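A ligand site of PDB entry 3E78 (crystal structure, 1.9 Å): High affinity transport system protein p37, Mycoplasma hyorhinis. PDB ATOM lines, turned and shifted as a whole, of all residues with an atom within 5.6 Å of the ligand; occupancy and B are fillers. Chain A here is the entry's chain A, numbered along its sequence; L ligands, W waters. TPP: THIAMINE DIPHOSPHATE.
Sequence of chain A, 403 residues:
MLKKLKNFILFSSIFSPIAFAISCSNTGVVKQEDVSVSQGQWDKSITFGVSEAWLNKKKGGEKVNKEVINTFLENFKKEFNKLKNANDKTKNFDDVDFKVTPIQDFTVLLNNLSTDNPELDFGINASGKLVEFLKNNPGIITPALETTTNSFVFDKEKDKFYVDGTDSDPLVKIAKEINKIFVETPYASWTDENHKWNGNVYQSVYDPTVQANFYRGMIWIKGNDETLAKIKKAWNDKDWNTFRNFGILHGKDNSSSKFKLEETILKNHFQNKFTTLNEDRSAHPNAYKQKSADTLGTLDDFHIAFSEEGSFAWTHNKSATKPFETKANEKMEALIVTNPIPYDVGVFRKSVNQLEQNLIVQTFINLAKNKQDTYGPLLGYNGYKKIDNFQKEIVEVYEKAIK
The side-chain hydroxyl (OG) of Ser 255 lies within hydrogen-bond range of the backbone NH (N) of Lys 258, at 2.9 Å.
The backbone carbonyl oxygen (O) of Gly 380 is in hydrogen-bond range of the side-chain hydroxyl (OG1) of Thr 149 (2.6 Å).
ND2 of Asn 200 sits at hydrogen-bond distance from O of Pro 377 (2.8 Å).
NZ of Lys 258 is in salt-bridge range of OE1 of Glu 308 (2.7 Å).
OH of Tyr 381 is in hydrogen-bond range of OD2 of Asp 344 (2.7 Å).
OG of Ser 257 is in hydrogen-bond range of NZ of Lys 258, at 3.3 Å.
The side-chain carboxylate (OD2) of Asp 344 lies close to a sulfur (S1) of the ligand (3.2 Å).
Merely in contact with the ligand: Leu 379 (3.1 Å), Val 201 (3.3 Å), Trp 314 (3.3 Å), Asn 200 (3.4 Å), Gly 380 (3.5 Å), Ala 126 (3.7 Å), Glu 308 (3.8 Å) and Pro 377 (3.8 Å).
Hydrophobic or aromatic side chains within 4 Å of the ligand: Ala 126, Val 201, Tyr 215, Trp 314 and Tyr 343.
Within 4 Å of the ligand: Ala 126, Lys 129, Asn 200, Val 201, Tyr 215, Ser 255, Ser 256, Ser 257, Lys 258, Glu 308, Trp 314, Tyr 343, Asp 344, Pro 377, Leu 379 and Gly 380.
The nearest printed residue that does not touch the ligand is Leu 378 (4.02 Å).
An oxygen (O1B) of the ligand sits at hydrogen-bond distance from the backbone NH (N) of Ser 257 (2.9 Å).
The side-chain amino group (NZ) of Lys 258 is in salt-bridge range of an oxygen (O1A) of the ligand, 2.8 Å away.
O2B of the ligand lies within salt-bridge range of NZ of Lys 129.
The backbone NH (N) of Ser 256 sits at hydrogen-bond distance from an oxygen (O2B) of the ligand.
An oxygen (O1B) of the ligand sits at hydrogen-bond distance from the side-chain hydroxyl (OH) of Tyr 215 (2.7 Å).
OG of Ser 257 lies within hydrogen-bond range of O1B of the ligand (2.6 Å).
The side-chain hydroxyl of Ser 255 is in hydrogen-bond range of an oxygen (O3B) of the ligand, 2.6 Å away.
The side-chain hydroxyl (OH) of Tyr 343 lies close to a sulfur (S1) of the ligand.
Water W1 lies within hydrogen-bond range of an oxygen (O2B) of the ligand (2.6 Å), the side-chain hydroxyl of Ser 256 (2.8 Å) and the backbone NH of Lys 129 (3.1 Å).
Water W7 bridges the side-chain hydroxyl (OH) of Tyr 206 (2.7 Å) and a nitrogen (N1') of the ligand (2.8 Å).
Water W6 bridges the side-chain carboxylate (OE1) of Glu 308 (2.7 Å) and an oxygen (O1A) of the ligand (2.8 Å).
Water W2 bridges OD2 of Asp 344 (2.6 Å) and O2A of the ligand (2.9 Å).
Water W5 bridges the side-chain amino group of Lys 129 (2.8 Å) and an oxygen (O2A) of the ligand (3.0 Å).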
ATOM      1  N   ALA A 126      10.427  26.622   5.358  1.00  0.00           N
ATOM      2  CA  ALA A 126      11.399  25.634   5.813  1.00  0.00           C
ATOM      3  C   ALA A 126      12.821  26.098   5.543  1.00  0.00           C
ATOM      4  O   ALA A 126      13.131  26.607   4.465  1.00  0.00           O
ATOM      5  CB  ALA A 126      11.173  24.285   5.134  1.00  0.00           C
ATOM      6  N   SER A 127      13.719  25.911   6.507  1.00  0.00           N
ATOM      7  CA  SER A 127      15.047  26.512   6.354  1.00  0.00           C
ATOM      8  C   SER A 127      15.802  25.894   5.191  1.00  0.00           C
ATOM      9  O   SER A 127      16.454  26.586   4.399  1.00  0.00           O
ATOM     10  CB  SER A 127      15.855  26.401   7.655  1.00  0.00           C
ATOM     11  OG  SER A 127      16.165  25.024   7.891  1.00  0.00           O
ATOM     12  N   LYS A 129      14.851  24.419   2.365  1.00  0.00           N
ATOM     13  CA  LYS A 129      14.348  24.871   1.067  1.00  0.00           C
ATOM     14  C   LYS A 129      14.723  26.321   0.802  1.00  0.00           C
ATOM     15  O   LYS A 129      15.006  26.775  -0.314  1.00  0.00           O
ATOM     16  CB  LYS A 129      12.829  24.727   1.056  1.00  0.00           C
ATOM     17  CG  LYS A 129      12.399  23.250   0.922  1.00  0.00           C
ATOM     18  CD  LYS A 129      10.919  23.137   1.242  1.00  0.00           C
ATOM     19  CE  LYS A 129      10.418  21.726   0.886  1.00  0.00           C
ATOM     20  NZ  LYS A 129       9.864  21.087   2.115  1.00  0.00           N
ATOM     21  N   THR A 149      11.212  25.564  18.528  1.00  0.00           N
ATOM     22  CA  THR A 149      10.121  24.644  18.863  1.00  0.00           C
ATOM     23  C   THR A 149      10.434  23.994  20.214  1.00  0.00           C
ATOM     24  O   THR A 149      11.596  23.912  20.608  1.00  0.00           O
ATOM     25  CB  THR A 149       9.968  23.647  17.702  1.00  0.00           C
ATOM     26  OG1 THR A 149       8.806  22.818  17.833  1.00  0.00           O
ATOM     27  CG2 THR A 149      11.138  22.685  17.629  1.00  0.00           C
ATOM     28  N   ASN A 200      -3.333  19.058  19.722  1.00  0.00           N
ATOM     29  CA  ASN A 200      -2.242  19.436  18.841  1.00  0.00           C
ATOM     30  C   ASN A 200      -1.061  18.462  18.857  1.00  0.00           C
ATOM     31  O   ASN A 200      -0.637  17.962  17.822  1.00  0.00           O
ATOM     32  CB  ASN A 200      -1.720  20.830  19.252  1.00  0.00           C
ATOM     33  CG  ASN A 200      -0.782  21.342  18.164  1.00  0.00           C
ATOM     34  OD1 ASN A 200      -1.006  21.006  17.001  1.00  0.00           O
ATOM     35  ND2 ASN A 200       0.219  22.110  18.557  1.00  0.00           N
ATOM     36  N   VAL A 201      -0.497  18.222  20.041  1.00  0.00           N
ATOM     37  CA  VAL A 201       0.666  17.358  20.218  1.00  0.00           C
ATOM     38  C   VAL A 201       0.521  16.517  21.486  1.00  0.00           C
ATOM     39  O   VAL A 201      -0.283  16.828  22.361  1.00  0.00           O
ATOM     40  CB  VAL A 201       1.984  18.160  20.305  1.00  0.00           C
ATOM     41  CG1 VAL A 201       2.166  19.064  19.103  1.00  0.00           C
ATOM     42  CG2 VAL A 201       2.043  18.954  21.604  1.00  0.00           C
ATOM     43  N   TYR A 206       7.649  16.166  25.204  1.00  0.00           N
ATOM     44  CA  TYR A 206       8.397  17.409  24.998  1.00  0.00           C
ATOM     45  C   TYR A 206       8.926  18.015  26.284  1.00  0.00           C
ATOM     46  O   TYR A 206       8.341  17.829  27.354  1.00  0.00           O
ATOM     47  CB  TYR A 206       7.477  18.474  24.392  1.00  0.00           C
ATOM     48  CG  TYR A 206       7.005  18.254  22.984  1.00  0.00           C
ATOM     49  CD1 TYR A 206       5.869  17.513  22.729  1.00  0.00           C
ATOM     50  CD2 TYR A 206       7.696  18.818  21.915  1.00  0.00           C
ATOM     51  CE1 TYR A 206       5.426  17.312  21.437  1.00  0.00           C
ATOM     52  CE2 TYR A 206       7.265  18.630  20.622  1.00  0.00           C
ATOM     53  CZ  TYR A 206       6.127  17.884  20.397  1.00  0.00           C
ATOM     54  OH  TYR A 206       5.690  17.693  19.097  1.00  0.00           O
ATOM     55  N   TYR A 215      15.742  20.923  14.008  1.00  0.00           N
ATOM     56  CA  TYR A 215      15.014  19.656  13.954  1.00  0.00           C
ATOM     57  C   TYR A 215      15.856  18.639  13.164  1.00  0.00           C
ATOM     58  O   TYR A 215      16.852  18.992  12.542  1.00  0.00           O
ATOM     59  CB  TYR A 215      13.633  19.753  13.357  1.00  0.00           C
ATOM     60  CG  TYR A 215      13.547  19.959  11.869  1.00  0.00           C
ATOM     61  CD1 TYR A 215      14.163  21.042  11.254  1.00  0.00           C
ATOM     62  CD2 TYR A 215      12.852  19.055  11.067  1.00  0.00           C
ATOM     63  CE1 TYR A 215      14.091  21.234   9.892  1.00  0.00           C
ATOM     64  CE2 TYR A 215      12.767  19.244   9.704  1.00  0.00           C
ATOM     65  CZ  TYR A 215      13.386  20.334   9.124  1.00  0.00           C
ATOM     66  OH  TYR A 215      13.305  20.503   7.765  1.00  0.00           O
ATOM     67  N   ASN A 254      12.863  17.285  -2.825  1.00  0.00           N
ATOM     68  CA  ASN A 254      13.344  18.568  -2.299  1.00  0.00           C
ATOM     69  C   ASN A 254      13.096  18.686  -0.797  1.00  0.00           C
ATOM     70  O   ASN A 254      13.288  19.736  -0.167  1.00  0.00           O
ATOM     71  CB  ASN A 254      12.685  19.700  -3.071  1.00  0.00           C
ATOM     72  CG  ASN A 254      11.185  19.744  -2.887  1.00  0.00           C
ATOM     73  OD1 ASN A 254      10.576  18.914  -2.212  1.00  0.00           O
ATOM     74  ND2 ASN A 254      10.529  20.743  -3.493  1.00  0.00           N
ATOM     75  N   SER A 255      12.681  17.604  -0.142  1.00  0.00           N
ATOM     76  CA  SER A 255      12.520  17.618   1.315  1.00  0.00           C
ATOM     77  C   SER A 255      13.823  17.428   2.062  1.00  0.00           C
ATOM     78  O   SER A 255      14.634  16.551   1.765  1.00  0.00           O
ATOM     79  CB  SER A 255      11.558  16.492   1.729  1.00  0.00           C
ATOM     80  OG  SER A 255      11.419  16.438   3.129  1.00  0.00           O
ATOM     81  N   SER A 256      14.069  18.242   3.084  1.00  0.00           N
ATOM     82  CA  SER A 256      15.229  18.037   3.925  1.00  0.00           C
ATOM     83  C   SER A 256      15.000  16.801   4.808  1.00  0.00           C
ATOM     84  O   SER A 256      15.806  15.864   4.750  1.00  0.00           O
ATOM     85  CB  SER A 256      15.499  19.250   4.819  1.00  0.00           C
ATOM     86  OG  SER A 256      15.822  20.376   4.009  1.00  0.00           O
ATOM     87  N   SER A 257      13.912  16.842   5.584  1.00  0.00           N
ATOM     88  CA  SER A 257      13.737  15.860   6.648  1.00  0.00           C
ATOM     89  C   SER A 257      13.148  14.537   6.144  1.00  0.00           C
ATOM     90  O   SER A 257      13.167  13.576   6.926  1.00  0.00           O
ATOM     91  CB  SER A 257      12.871  16.405   7.780  1.00  0.00           C
ATOM     92  OG  SER A 257      11.528  16.673   7.370  1.00  0.00           O
ATOM     93  N   LYS A 258      12.661  14.503   4.906  1.00  0.00           N
ATOM     94  CA  LYS A 258      12.085  13.259   4.362  1.00  0.00           C
ATOM     95  C   LYS A 258      12.870  12.813   3.139  1.00  0.00           C
ATOM     96  O   LYS A 258      12.495  11.890   2.407  1.00  0.00           O
ATOM     97  CB  LYS A 258      10.581  13.391   4.091  1.00  0.00           C
ATOM     98  CG  LYS A 258       9.784  13.624   5.362  1.00  0.00           C
ATOM     99  CD  LYS A 258       8.388  14.174   5.129  1.00  0.00           C
ATOM    100  CE  LYS A 258       8.454  15.647   4.743  1.00  0.00           C
ATOM    101  NZ  LYS A 258       8.592  16.520   5.923  1.00  0.00           N
ATOM    102  N   GLU A 308      10.234  13.069   9.544  1.00  0.00           N
ATOM    103  CA  GLU A 308      10.751  14.009  10.528  1.00  0.00           C
ATOM    104  C   GLU A 308      10.982  13.259  11.835  1.00  0.00           C
ATOM    105  O   GLU A 308      10.242  12.334  12.171  1.00  0.00           O
ATOM    106  CB  GLU A 308       9.763  15.137  10.821  1.00  0.00           C
ATOM    107  CG  GLU A 308       9.232  15.810   9.569  1.00  0.00           C
ATOM    108  CD  GLU A 308       8.061  15.102   8.929  1.00  0.00           C
ATOM    109  OE1 GLU A 308       7.313  15.821   8.220  1.00  0.00           O
ATOM    110  OE2 GLU A 308       7.834  13.894   9.092  1.00  0.00           O
ATOM    111  N   TRP A 314       3.009  14.579  16.971  1.00  0.00           N
ATOM    112  CA  TRP A 314       1.903  15.459  16.597  1.00  0.00           C
ATOM    113  C   TRP A 314       0.915  14.714  15.717  1.00  0.00           C
ATOM    114  O   TRP A 314       0.115  15.315  15.001  1.00  0.00           O
ATOM    115  CB  TRP A 314       2.407  16.732  15.907  1.00  0.00           C
ATOM    116  CG  TRP A 314       3.160  16.530  14.632  1.00  0.00           C
ATOM    117  CD1 TRP A 314       2.632  16.299  13.393  1.00  0.00           C
ATOM    118  CD2 TRP A 314       4.580  16.559  14.484  1.00  0.00           C
ATOM    119  NE1 TRP A 314       3.659  16.167  12.487  1.00  0.00           N
ATOM    120  CE2 TRP A 314       4.865  16.330  13.127  1.00  0.00           C
ATOM    121  CE3 TRP A 314       5.640  16.758  15.375  1.00  0.00           C
ATOM    122  CZ2 TRP A 314       6.158  16.289  12.600  1.00  0.00           C
ATOM    123  CZ3 TRP A 314       6.926  16.717  14.854  1.00  0.00           C
ATOM    124  CH2 TRP A 314       7.183  16.482  13.495  1.00  0.00           C
ATOM    125  N   TYR A 343      15.172  25.310  12.436  1.00  0.00           N
ATOM    126  CA  TYR A 343      13.726  25.310  12.273  1.00  0.00           C
ATOM    127  C   TYR A 343      13.306  26.402  11.284  1.00  0.00           C
ATOM    128  O   TYR A 343      14.184  26.977  10.647  1.00  0.00           O
ATOM    129  CB  TYR A 343      12.979  25.503  13.601  1.00  0.00           C
ATOM    130  CG  TYR A 343      11.839  24.515  13.746  1.00  0.00           C
ATOM    131  CD1 TYR A 343      10.532  24.952  13.911  1.00  0.00           C
ATOM    132  CD2 TYR A 343      12.071  23.139  13.698  1.00  0.00           C
ATOM    133  CE1 TYR A 343       9.489  24.056  14.039  1.00  0.00           C
ATOM    134  CE2 TYR A 343      11.030  22.233  13.828  1.00  0.00           C
ATOM    135  CZ  TYR A 343       9.738  22.696  13.998  1.00  0.00           C
ATOM    136  OH  TYR A 343       8.690  21.818  14.122  1.00  0.00           O
ATOM    137  N   ASP A 344      12.022  26.663  11.148  1.00  0.00           N
ATOM    138  CA  ASP A 344      11.556  27.454  10.001  1.00  0.00           C
ATOM    139  C   ASP A 344      11.986  28.931  10.135  1.00  0.00           C
ATOM    140  O   ASP A 344      12.218  29.443  11.227  1.00  0.00           O
ATOM    141  CB  ASP A 344      10.047  27.311   9.875  1.00  0.00           C
ATOM    142  CG  ASP A 344       9.656  25.898   9.432  1.00  0.00           C
ATOM    143  OD1 ASP A 344      10.534  25.025   9.294  1.00  0.00           O
ATOM    144  OD2 ASP A 344       8.448  25.689   9.210  1.00  0.00           O
ATOM    145  N   PRO A 377       2.168  27.873  17.739  1.00  0.00           N
ATOM    146  CA  PRO A 377       2.252  26.525  18.332  1.00  0.00           C
ATOM    147  C   PRO A 377       1.470  25.492  17.555  1.00  0.00           C
ATOM    148  O   PRO A 377       1.757  24.302  17.699  1.00  0.00           O
ATOM    149  CB  PRO A 377       1.622  26.693  19.722  1.00  0.00           C
ATOM    150  CG  PRO A 377       1.840  28.144  20.022  1.00  0.00           C
ATOM    151  CD  PRO A 377       1.586  28.813  18.697  1.00  0.00           C
ATOM    152  N   LEU A 378       0.510  25.937  16.757  1.00  0.00           N
ATOM    153  CA  LEU A 378      -0.265  25.012  15.934  1.00  0.00           C
ATOM    154  C   LEU A 378       0.618  24.453  14.820  1.00  0.00           C
ATOM    155  O   LEU A 378       0.302  23.436  14.184  1.00  0.00           O
ATOM    156  CB  LEU A 378      -1.515  25.684  15.352  1.00  0.00           C
ATOM    157  CG  LEU A 378      -2.595  26.094  16.358  1.00  0.00           C
ATOM    158  CD1 LEU A 378      -3.821  26.676  15.657  1.00  0.00           C
ATOM    159  CD2 LEU A 378      -3.010  24.906  17.225  1.00  0.00           C
ATOM    160  N   LEU A 379       1.729  25.136  14.584  1.00  0.00           N
ATOM    161  CA  LEU A 379       2.656  24.735  13.537  1.00  0.00           C
ATOM    162  C   LEU A 379       3.973  24.220  14.101  1.00  0.00           C
ATOM    163  O   LEU A 379       4.850  23.804  13.353  1.00  0.00           O
ATOM    164  CB  LEU A 379       2.944  25.925  12.611  1.00  0.00           C
ATOM    165  CG  LEU A 379       1.724  26.582  11.971  1.00  0.00           C
ATOM    166  CD1 LEU A 379       2.109  27.307  10.686  1.00  0.00           C
ATOM    167  CD2 LEU A 379       0.642  25.565  11.681  1.00  0.00           C
ATOM    168  N   GLY A 380       4.115  24.235  15.422  1.00  0.00           N
ATOM    169  CA  GLY A 380       5.389  23.781  15.971  1.00  0.00           C
ATOM    170  C   GLY A 380       6.265  24.950  16.369  1.00  0.00           C
ATOM    171  O   GLY A 380       7.368  24.777  16.844  1.00  0.00           O
ATOM    172  N   TYR A 381       5.777  26.176  16.158  1.00  0.00           N
ATOM    173  CA  TYR A 381       6.600  27.315  16.570  1.00  0.00           C
ATOM    174  C   TYR A 381       6.239  27.755  17.976  1.00  0.00           C
ATOM    175  O   TYR A 381       5.204  28.365  18.232  1.00  0.00           O
ATOM    176  CB  TYR A 381       6.407  28.485  15.610  1.00  0.00           C
ATOM    177  CG  TYR A 381       6.407  28.142  14.150  1.00  0.00           C
ATOM    178  CD1 TYR A 381       7.265  27.172  13.636  1.00  0.00           C
ATOM    179  CD2 TYR A 381       5.554  28.805  13.280  1.00  0.00           C
ATOM    180  CE1 TYR A 381       7.263  26.860  12.286  1.00  0.00           C
ATOM    181  CE2 TYR A 381       5.549  28.503  11.928  1.00  0.00           C
ATOM    182  CZ  TYR A 381       6.405  27.537  11.442  1.00  0.00           C
ATOM    183  OH  TYR A 381       6.384  27.241  10.087  1.00  0.00           O
HETATM  184  N1' TPP L   1       4.825  20.325  15.518  1.00  0.00           N
HETATM  185  C2' TPP L   1       3.517  20.521  15.239  1.00  0.00           C
HETATM  186  CM2 TPP L   1       2.519  20.864  16.338  1.00  0.00           C
HETATM  187  N3' TPP L   1       3.092  20.460  13.948  1.00  0.00           N
HETATM  188  C4' TPP L   1       3.982  20.159  12.973  1.00  0.00           C
HETATM  189  N4' TPP L   1       3.540  20.091  11.725  1.00  0.00           N
HETATM  190  C5' TPP L   1       5.339  19.942  13.248  1.00  0.00           C
HETATM  191  C6' TPP L   1       5.737  20.038  14.587  1.00  0.00           C
HETATM  192  C7' TPP L   1       6.398  19.600  12.192  1.00  0.00           C
HETATM  193  N3  TPP L   1       7.164  20.739  11.637  1.00  0.00           N
HETATM  194  C2  TPP L   1       6.655  21.980  11.637  1.00  0.00           C
HETATM  195  S1  TPP L   1       7.802  23.053  10.893  1.00  0.00           S
HETATM  196  C5  TPP L   1       8.950  21.780  10.580  1.00  0.00           C
HETATM  197  C4  TPP L   1       8.404  20.621  11.101  1.00  0.00           C
HETATM  198  CM4 TPP L   1       9.178  19.290  10.975  1.00  0.00           C
HETATM  199  C6  TPP L   1      10.342  22.075  10.009  1.00  0.00           C
HETATM  200  C7  TPP L   1      10.309  22.075   8.474  1.00  0.00           C
HETATM  201  O7  TPP L   1       9.844  20.784   8.045  1.00  0.00           O
HETATM  202  PA  TPP L   1       9.135  20.552   6.632  1.00  0.00           P
HETATM  203  O1A TPP L   1       8.508  19.212   6.632  1.00  0.00           O
HETATM  204  O2A TPP L   1       8.213  21.691   6.361  1.00  0.00           O
HETATM  205  O3A TPP L   1      10.259  20.679   5.551  1.00  0.00           O
HETATM  206  PB  TPP L   1      11.126  19.469   5.026  1.00  0.00           P
HETATM  207  O1B TPP L   1      11.935  18.872   6.133  1.00  0.00           O
HETATM  208  O2B TPP L   1      12.001  20.166   3.893  1.00  0.00           O
HETATM  209  O3B TPP L   1      10.189  18.377   4.341  1.00  0.00           O
HETATM  210  O   HOH W   1      13.706  22.145   4.180  1.00  0.00           O
HETATM  211  O   HOH W   2       7.287  24.276   7.330  1.00  0.00           O
HETATM  212  O   HOH W   3       4.621  20.471   8.864  1.00  0.00           O
HETATM  213  O   HOH W   4       0.484  19.839  13.319  1.00  0.00           O
HETATM  214  O   HOH W   5       8.221  22.788   3.546  1.00  0.00           O
HETATM  215  O   HOH W   6       6.600  18.443   8.538  1.00  0.00           O
HETATM  216  O   HOH W   7       6.174  20.062  17.950  1.00  0.00           O
